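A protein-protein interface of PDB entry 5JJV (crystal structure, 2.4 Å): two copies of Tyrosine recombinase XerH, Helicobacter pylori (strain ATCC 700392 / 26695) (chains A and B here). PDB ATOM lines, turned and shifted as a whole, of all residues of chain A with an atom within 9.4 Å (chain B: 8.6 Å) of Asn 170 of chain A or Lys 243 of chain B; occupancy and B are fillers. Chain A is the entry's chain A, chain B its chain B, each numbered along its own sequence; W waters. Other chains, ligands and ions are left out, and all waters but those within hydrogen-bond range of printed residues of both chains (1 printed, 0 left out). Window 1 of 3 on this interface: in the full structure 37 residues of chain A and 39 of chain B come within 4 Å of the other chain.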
ATOM      1  N   SER A 122       6.959 -13.579  -3.796  1.00  0.00           N
ATOM      2  CA  SER A 122       6.318 -12.364  -4.287  1.00  0.00           C
ATOM      3  C   SER A 122       5.537 -11.671  -3.176  1.00  0.00           C
ATOM      4  O   SER A 122       5.168 -12.298  -2.181  1.00  0.00           O
ATOM      5  CB  SER A 122       5.389 -12.679  -5.462  1.00  0.00           C
ATOM      6  OG  SER A 122       4.266 -13.432  -5.039  1.00  0.00           O
ATOM      7  N   LEU A 123       5.290 -10.376  -3.352  1.00  0.00           N
ATOM      8  CA  LEU A 123       4.550  -9.599  -2.365  1.00  0.00           C
ATOM      9  C   LEU A 123       3.111 -10.089  -2.254  1.00  0.00           C
ATOM     10  O   LEU A 123       2.507 -10.025  -1.183  1.00  0.00           O
ATOM     11  CB  LEU A 123       4.577  -8.111  -2.720  1.00  0.00           C
ATOM     12  CG  LEU A 123       5.947  -7.433  -2.648  1.00  0.00           C
ATOM     13  CD1 LEU A 123       5.822  -5.939  -2.893  1.00  0.00           C
ATOM     14  CD2 LEU A 123       6.616  -7.706  -1.309  1.00  0.00           C
ATOM     15  N   ALA A 124       2.571 -10.581  -3.363  1.00  0.00           N
ATOM     16  CA  ALA A 124       1.224 -11.136  -3.377  1.00  0.00           C
ATOM     17  C   ALA A 124       1.154 -12.394  -2.519  1.00  0.00           C
ATOM     18  O   ALA A 124       0.163 -12.632  -1.827  1.00  0.00           O
ATOM     19  CB  ALA A 124       0.788 -11.437  -4.799  1.00  0.00           C
ATOM     20  N   LYS A 127       1.206 -11.491   1.167  1.00  0.00           N
ATOM     21  CA  LYS A 127      -0.123 -11.094   1.619  1.00  0.00           C
ATOM     22  C   LYS A 127      -0.977 -12.311   1.956  1.00  0.00           C
ATOM     23  O   LYS A 127      -1.717 -12.301   2.939  1.00  0.00           O
ATOM     24  CB  LYS A 127      -0.819 -10.236   0.559  1.00  0.00           C
ATOM     25  CG  LYS A 127      -0.136  -8.900   0.298  1.00  0.00           C
ATOM     26  CD  LYS A 127      -0.893  -8.075  -0.735  1.00  0.00           C
ATOM     27  CE  LYS A 127      -0.204  -6.743  -0.998  1.00  0.00           C
ATOM     28  NZ  LYS A 127      -1.022  -5.859  -1.873  1.00  0.00           N
ATOM     29  N   GLY A 163       4.522  -3.889   2.418  1.00  0.00           N
ATOM     30  CA  GLY A 163       3.892  -4.457   1.239  1.00  0.00           C
ATOM     31  C   GLY A 163       2.684  -5.329   1.525  1.00  0.00           C
ATOM     32  O   GLY A 163       2.535  -6.401   0.937  1.00  0.00           O
ATOM     33  N   VAL A 164       1.816  -4.870   2.420  1.00  0.00           N
ATOM     34  CA  VAL A 164       0.643  -5.648   2.801  1.00  0.00           C
ATOM     35  C   VAL A 164      -0.650  -4.978   2.348  1.00  0.00           C
ATOM     36  O   VAL A 164      -1.652  -5.648   2.091  1.00  0.00           O
ATOM     37  CB  VAL A 164       0.598  -5.878   4.326  1.00  0.00           C
ATOM     38  CG1 VAL A 164       1.863  -6.582   4.777  1.00  0.00           C
ATOM     39  CG2 VAL A 164       0.426  -4.561   5.074  1.00  0.00           C
ATOM     40  N   ASN A 165      -0.621  -3.654   2.245  1.00  0.00           N
ATOM     41  CA  ASN A 165      -1.784  -2.892   1.825  1.00  0.00           C
ATOM     42  C   ASN A 165      -1.939  -2.914   0.313  1.00  0.00           C
ATOM     43  O   ASN A 165      -1.095  -3.460  -0.397  1.00  0.00           O
ATOM     44  CB  ASN A 165      -1.681  -1.451   2.321  1.00  0.00           C
ATOM     45  CG  ASN A 165      -0.379  -0.788   1.912  1.00  0.00           C
ATOM     46  OD1 ASN A 165       0.607  -0.824   2.649  1.00  0.00           O
ATOM     47  ND2 ASN A 165      -0.368  -0.179   0.732  1.00  0.00           N
ATOM     48  N   GLN A 166      -3.022  -2.320  -0.176  1.00  0.00           N
ATOM     49  CA  GLN A 166      -3.195  -2.131  -1.610  1.00  0.00           C
ATOM     50  C   GLN A 166      -2.152  -1.133  -2.102  1.00  0.00           C
ATOM     51  O   GLN A 166      -1.509  -0.457  -1.296  1.00  0.00           O
ATOM     52  CB  GLN A 166      -4.608  -1.648  -1.935  1.00  0.00           C
ATOM     53  N   SER A 167      -1.983  -1.062  -3.420  1.00  0.00           N
ATOM     54  CA  SER A 167      -0.983  -0.206  -4.070  1.00  0.00           C
ATOM     55  C   SER A 167       0.456  -0.644  -3.774  1.00  0.00           C
ATOM     56  O   SER A 167       1.405  -0.075  -4.313  1.00  0.00           O
ATOM     57  CB  SER A 167      -1.170   1.264  -3.675  1.00  0.00           C
ATOM     58  OG  SER A 167      -0.753   1.498  -2.340  1.00  0.00           O
ATOM     59  N   ALA A 168       0.614  -1.658  -2.928  1.00  0.00           N
ATOM     60  CA  ALA A 168       1.931  -2.190  -2.601  1.00  0.00           C
ATOM     61  C   ALA A 168       2.128  -3.550  -3.258  1.00  0.00           C
ATOM     62  O   ALA A 168       1.589  -4.557  -2.799  1.00  0.00           O
ATOM     63  CB  ALA A 168       2.106  -2.293  -1.095  1.00  0.00           C
ATOM     64  N   GLY A 169       2.903  -3.573  -4.336  1.00  0.00           N
ATOM     65  CA  GLY A 169       3.092  -4.788  -5.104  1.00  0.00           C
ATOM     66  C   GLY A 169       1.900  -5.043  -6.004  1.00  0.00           C
ATOM     67  O   GLY A 169       1.711  -6.150  -6.507  1.00  0.00           O
ATOM     68  N   ASN A 170       1.091  -4.006  -6.203  1.00  0.00           N
ATOM     69  CA  ASN A 170      -0.083  -4.093  -7.062  1.00  0.00           C
ATOM     70  C   ASN A 170       0.304  -4.129  -8.536  1.00  0.00           C
ATOM     71  O   ASN A 170      -0.037  -3.230  -9.304  1.00  0.00           O
ATOM     72  CB  ASN A 170      -1.028  -2.917  -6.793  1.00  0.00           C
ATOM     73  CG  ASN A 170      -0.373  -1.571  -7.049  1.00  0.00           C
ATOM     74  OD1 ASN A 170       0.848  -1.436  -6.979  1.00  0.00           O
ATOM     75  ND2 ASN A 170      -1.187  -0.567  -7.354  1.00  0.00           N
ATOM     76  N   LYS A 171       1.021  -5.181  -8.918  1.00  0.00           N
ATOM     77  CA  LYS A 171       1.525  -5.331 -10.278  1.00  0.00           C
ATOM     78  C   LYS A 171       0.419  -5.151 -11.311  1.00  0.00           C
ATOM     79  O   LYS A 171      -0.547  -5.917 -11.334  1.00  0.00           O
ATOM     80  CB  LYS A 171       2.186  -6.701 -10.448  1.00  0.00           C
ATOM     81  CG  LYS A 171       3.180  -7.042  -9.351  1.00  0.00           C
ATOM     82  CD  LYS A 171       3.708  -8.461  -9.485  1.00  0.00           C
ATOM     83  CE  LYS A 171       4.545  -8.630 -10.739  1.00  0.00           C
ATOM     84  NZ  LYS A 171       5.208  -9.963 -10.780  1.00  0.00           N
ATOM     85  N   LEU A 172       0.552  -4.120 -12.141  1.00  0.00           N
ATOM     86  CA  LEU A 172      -0.373  -3.903 -13.245  1.00  0.00           C
ATOM     87  C   LEU A 172      -0.404  -5.152 -14.113  1.00  0.00           C
ATOM     88  O   LEU A 172       0.647  -5.676 -14.484  1.00  0.00           O
ATOM     89  CB  LEU A 172       0.030  -2.680 -14.070  1.00  0.00           C
ATOM     90  CG  LEU A 172      -0.097  -1.321 -13.379  1.00  0.00           C
ATOM     91  CD1 LEU A 172       0.395  -0.207 -14.288  1.00  0.00           C
ATOM     92  CD2 LEU A 172      -1.535  -1.071 -12.954  1.00  0.00           C
ATOM     93  N   PRO A 173      -1.613  -5.642 -14.421  1.00  0.00           N
ATOM     94  CA  PRO A 173      -1.794  -6.914 -15.127  1.00  0.00           C
ATOM     95  C   PRO A 173      -1.096  -6.953 -16.483  1.00  0.00           C
ATOM     96  O   PRO A 173      -1.317  -6.080 -17.320  1.00  0.00           O
ATOM     97  CB  PRO A 173      -3.316  -7.013 -15.294  1.00  0.00           C
ATOM     98  CG  PRO A 173      -3.820  -5.620 -15.133  1.00  0.00           C
ATOM     99  CD  PRO A 173      -2.898  -4.976 -14.150  1.00  0.00           C
ATOM    100  N   THR A 174      -0.249  -7.960 -16.673  1.00  0.00           N
ATOM    101  CA  THR A 174       0.414  -8.187 -17.949  1.00  0.00           C
ATOM    102  C   THR A 174      -0.628  -8.484 -19.019  1.00  0.00           C
ATOM    103  O   THR A 174      -1.580  -9.226 -18.775  1.00  0.00           O
ATOM    104  CB  THR A 174       1.420  -9.352 -17.858  1.00  0.00           C
ATOM    105  OG1 THR A 174       2.397  -9.064 -16.850  1.00  0.00           O
ATOM    106  CG2 THR A 174       2.120  -9.570 -19.189  1.00  0.00           C
ATOM    107  N   ASN A 340     -13.531  -1.505  -8.303  1.00  0.00           N
ATOM    108  CA  ASN A 340     -12.117  -1.406  -7.969  1.00  0.00           C
ATOM    109  C   ASN A 340     -11.279  -2.212  -8.949  1.00  0.00           C
ATOM    110  O   ASN A 340     -10.193  -1.795  -9.347  1.00  0.00           O
ATOM    111  CB  ASN A 340     -11.864  -1.887  -6.539  1.00  0.00           C
ATOM    112  CG  ASN A 340     -12.547  -1.022  -5.500  1.00  0.00           C
ATOM    113  OD1 ASN A 340     -12.750   0.174  -5.711  1.00  0.00           O
ATOM    114  ND2 ASN A 340     -12.902  -1.621  -4.369  1.00  0.00           N
ATOM    115  N   ILE A 344      -8.726  -0.707 -12.509  1.00  0.00           N
ATOM    116  CA  ILE A 344      -7.324  -1.062 -12.730  1.00  0.00           C
ATOM    117  C   ILE A 344      -6.884  -0.775 -14.163  1.00  0.00           C
ATOM    118  O   ILE A 344      -5.769  -0.310 -14.407  1.00  0.00           O
ATOM    119  CB  ILE A 344      -7.071  -2.556 -12.421  1.00  0.00           C
ATOM    120  CG1 ILE A 344      -7.302  -2.847 -10.938  1.00  0.00           C
ATOM    121  CG2 ILE A 344      -5.661  -2.967 -12.822  1.00  0.00           C
ATOM    122  CD1 ILE A 344      -7.129  -4.303 -10.576  1.00  0.00           C
ATOM    123  N   HIS A 347      -5.445   2.576 -15.853  1.00  0.00           N
ATOM    124  CA  HIS A 347      -4.034   2.932 -15.750  1.00  0.00           C
ATOM    125  C   HIS A 347      -3.315   2.811 -17.091  1.00  0.00           C
ATOM    126  O   HIS A 347      -2.188   3.283 -17.242  1.00  0.00           O
ATOM    127  CB  HIS A 347      -3.334   2.055 -14.707  1.00  0.00           C
ATOM    128  CG  HIS A 347      -3.790   2.304 -13.303  1.00  0.00           C
ATOM    129  ND1 HIS A 347      -2.974   2.867 -12.344  1.00  0.00           N
ATOM    130  CD2 HIS A 347      -4.975   2.066 -12.694  1.00  0.00           C
ATOM    131  CE1 HIS A 347      -3.638   2.965 -11.207  1.00  0.00           C
ATOM    132  NE2 HIS A 347      -4.855   2.486 -11.392  1.00  0.00           N
ATOM    133  N   PHE A 348      -3.967   2.177 -18.061  1.00  0.00           N
ATOM    134  CA  PHE A 348      -3.381   2.002 -19.386  1.00  0.00           C
ATOM    135  C   PHE A 348      -4.028   2.928 -20.410  1.00  0.00           C
ATOM    136  O   PHE A 348      -3.794   2.796 -21.611  1.00  0.00           O
ATOM    137  CB  PHE A 348      -3.517   0.550 -19.849  1.00  0.00           C
ATOM    138  CG  PHE A 348      -2.992  -0.454 -18.866  1.00  0.00           C
ATOM    139  CD1 PHE A 348      -1.630  -0.574 -18.639  1.00  0.00           C
ATOM    140  CD2 PHE A 348      -3.858  -1.289 -18.180  1.00  0.00           C
ATOM    141  CE1 PHE A 348      -1.144  -1.500 -17.737  1.00  0.00           C
ATOM    142  CE2 PHE A 348      -3.377  -2.218 -17.278  1.00  0.00           C
ATOM    143  CZ  PHE A 348      -2.018  -2.324 -17.056  1.00  0.00           C
ATOM    144  N   SER B  34      12.638  -5.242  -0.770  1.00  0.00           N
ATOM    145  CA  SER B  34      12.532  -5.295  -2.227  1.00  0.00           C
ATOM    146  C   SER B  34      13.863  -5.025  -2.923  1.00  0.00           C
ATOM    147  O   SER B  34      14.121  -5.550  -4.005  1.00  0.00           O
ATOM    148  CB  SER B  34      11.483  -4.295  -2.717  1.00  0.00           C
ATOM    149  OG  SER B  34      10.199  -4.615  -2.212  1.00  0.00           O
ATOM    150  N   ARG B 214      11.842   8.496 -11.353  1.00  0.00           N
ATOM    151  CA  ARG B 214      12.813   8.510 -10.261  1.00  0.00           C
ATOM    152  C   ARG B 214      14.137   7.906 -10.718  1.00  0.00           C
ATOM    153  O   ARG B 214      14.197   7.232 -11.748  1.00  0.00           O
ATOM    154  CB  ARG B 214      12.288   7.747  -9.043  1.00  0.00           C
ATOM    155  CG  ARG B 214      11.134   8.412  -8.305  1.00  0.00           C
ATOM    156  CD  ARG B 214      10.857   7.681  -6.997  1.00  0.00           C
ATOM    157  NE  ARG B 214       9.712   8.218  -6.268  1.00  0.00           N
ATOM    158  CZ  ARG B 214       8.461   7.802  -6.434  1.00  0.00           C
ATOM    159  NH1 ARG B 214       8.191   6.847  -7.314  1.00  0.00           N
ATOM    160  NH2 ARG B 214       7.478   8.340  -5.722  1.00  0.00           N
ATOM    161  N   GLU B 217      14.180   4.047 -10.576  1.00  0.00           N
ATOM    162  CA  GLU B 217      13.197   3.597 -11.556  1.00  0.00           C
ATOM    163  C   GLU B 217      13.799   3.589 -12.958  1.00  0.00           C
ATOM    164  O   GLU B 217      13.498   2.713 -13.769  1.00  0.00           O
ATOM    165  CB  GLU B 217      11.954   4.488 -11.523  1.00  0.00           C
ATOM    166  CG  GLU B 217      11.163   4.411 -10.230  1.00  0.00           C
ATOM    167  CD  GLU B 217      10.040   5.426 -10.179  1.00  0.00           C
ATOM    168  OE1 GLU B 217       9.960   6.268 -11.097  1.00  0.00           O
ATOM    169  OE2 GLU B 217       9.240   5.387  -9.220  1.00  0.00           O
ATOM    170  N   LEU B 236       6.249   0.601 -18.414  1.00  0.00           N
ATOM    171  CA  LEU B 236       5.820   0.109 -17.111  1.00  0.00           C
ATOM    172  C   LEU B 236       6.915   0.330 -16.074  1.00  0.00           C
ATOM    173  O   LEU B 236       8.063  -0.065 -16.278  1.00  0.00           O
ATOM    174  CB  LEU B 236       5.446  -1.372 -17.182  1.00  0.00           C
ATOM    175  CG  LEU B 236       4.126  -1.695 -17.882  1.00  0.00           C
ATOM    176  CD1 LEU B 236       3.838  -3.188 -17.830  1.00  0.00           C
ATOM    177  CD2 LEU B 236       2.985  -0.905 -17.262  1.00  0.00           C
ATOM    178  N   ILE B 237       6.552   0.966 -14.965  1.00  0.00           N
ATOM    179  CA  ILE B 237       7.517   1.302 -13.926  1.00  0.00           C
ATOM    180  C   ILE B 237       7.185   0.660 -12.584  1.00  0.00           C
ATOM    181  O   ILE B 237       6.111   0.889 -12.027  1.00  0.00           O
ATOM    182  CB  ILE B 237       7.606   2.825 -13.713  1.00  0.00           C
ATOM    183  CG1 ILE B 237       8.084   3.525 -14.983  1.00  0.00           C
ATOM    184  CG2 ILE B 237       8.535   3.148 -12.553  1.00  0.00           C
ATOM    185  CD1 ILE B 237       8.194   5.022 -14.827  1.00  0.00           C
ATOM    186  N   LYS B 238       8.112  -0.143 -12.072  1.00  0.00           N
ATOM    187  CA  LYS B 238       8.040  -0.607 -10.693  1.00  0.00           C
ATOM    188  C   LYS B 238       8.613   0.487  -9.801  1.00  0.00           C
ATOM    189  O   LYS B 238       9.830   0.625  -9.679  1.00  0.00           O
ATOM    190  CB  LYS B 238       8.805  -1.920 -10.512  1.00  0.00           C
ATOM    191  CG  LYS B 238       8.798  -2.469  -9.091  1.00  0.00           C
ATOM    192  CD  LYS B 238       9.501  -3.819  -9.023  1.00  0.00           C
ATOM    193  CE  LYS B 238       9.495  -4.391  -7.615  1.00  0.00           C
ATOM    194  NZ  LYS B 238      10.378  -3.631  -6.686  1.00  0.00           N
ATOM    195  N   GLY B 239       7.730   1.273  -9.191  1.00  0.00           N
ATOM    196  CA  GLY B 239       8.141   2.467  -8.478  1.00  0.00           C
ATOM    197  C   GLY B 239       8.451   2.281  -7.005  1.00  0.00           C
ATOM    198  O   GLY B 239       8.507   1.158  -6.503  1.00  0.00           O
ATOM    199  N   LYS B 240       8.661   3.403  -6.321  1.00  0.00           N
ATOM    200  CA  LYS B 240       8.953   3.417  -4.893  1.00  0.00           C
ATOM    201  C   LYS B 240       7.828   2.760  -4.099  1.00  0.00           C
ATOM    202  O   LYS B 240       6.651   3.011  -4.355  1.00  0.00           O
ATOM    203  CB  LYS B 240       9.175   4.855  -4.418  1.00  0.00           C
ATOM    204  CG  LYS B 240       9.366   5.005  -2.919  1.00  0.00           C
ATOM    205  CD  LYS B 240       9.450   6.473  -2.528  1.00  0.00           C
ATOM    206  CE  LYS B 240       9.596   6.638  -1.023  1.00  0.00           C
ATOM    207  NZ  LYS B 240       9.551   8.070  -0.623  1.00  0.00           N
ATOM    208  N   GLY B 241       8.193   1.914  -3.142  1.00  0.00           N
ATOM    209  CA  GLY B 241       7.206   1.182  -2.370  1.00  0.00           C
ATOM    210  C   GLY B 241       6.533   0.115  -3.211  1.00  0.00           C
ATOM    211  O   GLY B 241       5.425  -0.327  -2.899  1.00  0.00           O
ATOM    212  N   ASP B 242       7.210  -0.287  -4.285  1.00  0.00           N
ATOM    213  CA  ASP B 242       6.720  -1.316  -5.199  1.00  0.00           C
ATOM    214  C   ASP B 242       5.377  -0.942  -5.823  1.00  0.00           C
ATOM    215  O   ASP B 242       4.567  -1.814  -6.143  1.00  0.00           O
ATOM    216  CB  ASP B 242       6.615  -2.660  -4.474  1.00  0.00           C
ATOM    217  CG  ASP B 242       7.946  -3.118  -3.912  1.00  0.00           C
ATOM    218  OD1 ASP B 242       8.949  -3.079  -4.655  1.00  0.00           O
ATOM    219  OD2 ASP B 242       7.993  -3.503  -2.724  1.00  0.00           O
ATOM    220  N   LYS B 243       5.152   0.357  -5.994  1.00  0.00           N
ATOM    221  CA  LYS B 243       3.945   0.855  -6.645  1.00  0.00           C
ATOM    222  C   LYS B 243       4.140   0.874  -8.156  1.00  0.00           C
ATOM    223  O   LYS B 243       5.062   1.513  -8.661  1.00  0.00           O
ATOM    224  CB  LYS B 243       3.595   2.260  -6.146  1.00  0.00           C
ATOM    225  CG  LYS B 243       3.467   2.384  -4.636  1.00  0.00           C
ATOM    226  CD  LYS B 243       3.385   3.848  -4.222  1.00  0.00           C
ATOM    227  CE  LYS B 243       3.313   4.005  -2.711  1.00  0.00           C
ATOM    228  NZ  LYS B 243       2.021   3.515  -2.157  1.00  0.00           N
ATOM    229  N   TYR B 244       3.274   0.173  -8.877  1.00  0.00           N
ATOM    230  CA  TYR B 244       3.387   0.114 -10.329  1.00  0.00           C
ATOM    231  C   TYR B 244       2.579   1.210 -11.007  1.00  0.00           C
ATOM    232  O   TYR B 244       1.481   1.553 -10.569  1.00  0.00           O
ATOM    233  CB  TYR B 244       2.946  -1.255 -10.847  1.00  0.00           C
ATOM    234  CG  TYR B 244       3.968  -2.341 -10.619  1.00  0.00           C
ATOM    235  CD1 TYR B 244       4.057  -2.993  -9.397  1.00  0.00           C
ATOM    236  CD2 TYR B 244       4.849  -2.712 -11.626  1.00  0.00           C
ATOM    237  CE1 TYR B 244       4.992  -3.985  -9.184  1.00  0.00           C
ATOM    238  CE2 TYR B 244       5.788  -3.704 -11.423  1.00  0.00           C
ATOM    239  CZ  TYR B 244       5.855  -4.338 -10.201  1.00  0.00           C
ATOM    240  OH  TYR B 244       6.790  -5.328  -9.996  1.00  0.00           O
ATOM    241  N   ARG B 245       3.137   1.757 -12.080  1.00  0.00           N
ATOM    242  CA  ARG B 245       2.450   2.764 -12.872  1.00  0.00           C
ATOM    243  C   ARG B 245       2.976   2.747 -14.300  1.00  0.00           C
ATOM    244  O   ARG B 245       4.100   2.314 -14.552  1.00  0.00           O
ATOM    245  CB  ARG B 245       2.624   4.156 -12.259  1.00  0.00           C
ATOM    246  CG  ARG B 245       4.022   4.735 -12.408  1.00  0.00           C
ATOM    247  CD  ARG B 245       4.106   6.134 -11.818  1.00  0.00           C
ATOM    248  NE  ARG B 245       5.373   6.788 -12.137  1.00  0.00           N
ATOM    249  CZ  ARG B 245       6.473   6.683 -11.400  1.00  0.00           C
ATOM    250  NH1 ARG B 245       7.581   7.312 -11.766  1.00  0.00           N
ATOM    251  NH2 ARG B 245       6.465   5.947 -10.296  1.00  0.00           N
ATOM    252  N   ALA B 246       2.152   3.208 -15.234  1.00  0.00           N
ATOM    253  CA  ALA B 246       2.564   3.301 -16.627  1.00  0.00           C
ATOM    254  C   ALA B 246       2.777   4.758 -17.007  1.00  0.00           C
ATOM    255  O   ALA B 246       1.970   5.621 -16.663  1.00  0.00           O
ATOM    256  CB  ALA B 246       1.530   2.655 -17.537  1.00  0.00           C
ATOM    257  N   LEU B 334       3.450  10.774 -11.467  1.00  0.00           N
ATOM    258  CA  LEU B 334       4.494  10.653 -10.456  1.00  0.00           C
ATOM    259  C   LEU B 334       4.291   9.424  -9.576  1.00  0.00           C
ATOM    260  O   LEU B 334       5.228   8.944  -8.941  1.00  0.00           O
ATOM    261  CB  LEU B 334       4.548  11.915  -9.590  1.00  0.00           C
ATOM    262  CG  LEU B 334       5.493  13.041 -10.021  1.00  0.00           C
ATOM    263  CD1 LEU B 334       5.294  13.418 -11.480  1.00  0.00           C
ATOM    264  CD2 LEU B 334       5.300  14.257  -9.126  1.00  0.00           C
ATOM    265  N   GLY B 335       3.062   8.919  -9.543  1.00  0.00           N
ATOM    266  CA  GLY B 335       2.740   7.758  -8.736  1.00  0.00           C
ATOM    267  C   GLY B 335       2.501   8.116  -7.282  1.00  0.00           C
ATOM    268  O   GLY B 335       3.145   7.574  -6.384  1.00  0.00           O
ATOM    269  N   HIS B 336       1.572   9.038  -7.051  1.00  0.00           N
ATOM    270  CA  HIS B 336       1.239   9.467  -5.698  1.00  0.00           C
ATOM    271  C   HIS B 336      -0.190   9.085  -5.337  1.00  0.00           C
ATOM    272  O   HIS B 336      -0.978   8.703  -6.201  1.00  0.00           O
ATOM    273  CB  HIS B 336       1.434  10.975  -5.550  1.00  0.00           C
ATOM    274  CG  HIS B 336       2.869  11.403  -5.571  1.00  0.00           C
ATOM    275  ND1 HIS B 336       3.260  12.680  -5.913  1.00  0.00           N
ATOM    276  CD2 HIS B 336       4.005  10.725  -5.289  1.00  0.00           C
ATOM    277  CE1 HIS B 336       4.576  12.768  -5.844  1.00  0.00           C
ATOM    278  NE2 HIS B 336       5.053  11.595  -5.467  1.00  0.00           N
ATOM    279  N   ALA B 337      -0.518   9.193  -4.055  1.00  0.00           N
ATOM    280  CA  ALA B 337      -1.837   8.813  -3.569  1.00  0.00           C
ATOM    281  C   ALA B 337      -2.689  10.035  -3.244  1.00  0.00           C
ATOM    282  O   ALA B 337      -3.916   9.950  -3.200  1.00  0.00           O
ATOM    283  CB  ALA B 337      -1.709   7.918  -2.346  1.00  0.00           C
HETATM  284  O   HOH W   1      -0.334   4.067 -14.705  1.00  0.00           O
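The side-chain amino group (NZ) of Lys 243 of chain B is in hydrogen-bond range of the side-chain hydroxyl (OG) of Ser 167 of chain A. N of Gly 169 of chain A is in hydrogen-bond range of O of Asp 242 of chain B (3.0 Å). OD1 of Asn 170 of chain A is in hydrogen-bond range of N of Tyr 244 of chain B, 3.5 Å away.
The side-chain amino group (NZ) of Lys 127 of chain A lies within hydrogen-bond range of the backbone carbonyl oxygen (O) of Ala 168 of chain A (3.1 Å). The side-chain amide oxygen (OD1) of Asn 170 of chain A lies close to the backbone carbonyl oxygen (O) of Ser 167 of chain A (3.0 Å). The side-chain hydroxyl of Ser 34 of chain B lies within hydrogen-bond range of the side-chain carboxylate of Asp 242 of chain B, 2.5 Å away. OE1 of Glu 217 of chain B is in salt-bridge range of NH1 of Arg 245 of chain B (2.7 Å). The backbone NH (N) of Ile 237 of chain B sits at hydrogen-bond distance from the backbone carbonyl oxygen (O) of Arg 245 of chain B. The side-chain amino group (NZ) of Lys 238 of chain B is in salt-bridge range of the side-chain carboxylate (OD1) of Asp 242 of chain B (2.5 Å).
Among the printed residues, merely in contact across the chains: Leu 123 of chain A with Asp 242 of chain B (3.3 Å), Lys 171 of chain A with Tyr 244 of chain B (3.6 Å), His 347 of chain A with Ala 246 of chain B (3.8 Å), Asn 170 of chain A with Asp 242 of chain B (3.8 Å), Asn 170 of chain A with Lys 243 of chain B (3.9 Å), Leu 172 of chain A with Arg 245 of chain B (3.9 Å), Leu 172 of chain A with Tyr 244 of chain B (3.95 Å), Leu 172 of chain A with Ala 246 of chain B (3.96 Å) and Ala 168 of chain A with Gly 241 of chain B (3.97 Å).
Lys 127 of chain A touches none of the printed residues of chain B. Of chain B, only Lys 243 comes within 4 Å of Ser 167 of chain A. Printed residues of chain B within 4 Å of Gly 169 of chain A: Asp 242 (3.0 Å). Of chain B, only Asp 242 (3.8 Å), Lys 243 (3.9 Å) and Tyr 244 (3.5 Å) come within 4 Å of Asn 170 of chain A. Asn 340 of chain A touches none of the printed residues of chain B. Printed residues of chain B within 4 Å of His 347 of chain A: Ala 246. No residue of chain A comes within 4 Å of Gly 239 of chain B. Gly 241 of chain B touches one residue of chain A. Of the printed residues of chain A, Lys 243 of chain B touches Ser 167 and Asn 170. Of the printed residues of chain A, Tyr 244 of chain B touches Asn 170, Lys 171 and Leu 172. Of the printed residues of chain A, Arg 245 of chain B touches Leu 172 (3.9 Å). The nearest residue of chain A that does not touch Lys 243 of chain B is Gly 169 of chain A (4.8 Å). The nearest printed residue of chain B that does not touch Lys 171 of chain A is Asp 242 of chain B (5.6 Å).
Of the 20 printed residues of chain A, 8 touch a printed residue of chain B. Printed residues of chain A that touch a printed residue of chain B: Leu 123, Ser 167, Ala 168, Gly 169, Asn 170, Lys 171, Leu 172 and His 347. Hydrophobic or aromatic side chains of chain A that line the printed part of chain B: Leu 123 and Leu 172. Of the 18 printed residues of chain B, 6 touch a printed residue of chain A. Hydrophobic or aromatic side chains of chain B that line the printed part of chain A: Tyr 244 and Ala 246. Among the printed residues, 12 pairs touch across the chains. Among the printed residues, no Asp or Glu carboxylate lies within 4 Å of a Lys or Arg side-chain nitrogen of the other chain.
No position is printed for both chains. Of the 12 pairs that touch across the chains among the printed residues, none has its exchanged pair printed and touching as well.
Water W1 lies within hydrogen-bond range of N of Ala 246 of chain B (2.7 Å) and O of His 347 of chain A (3.2 Å).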
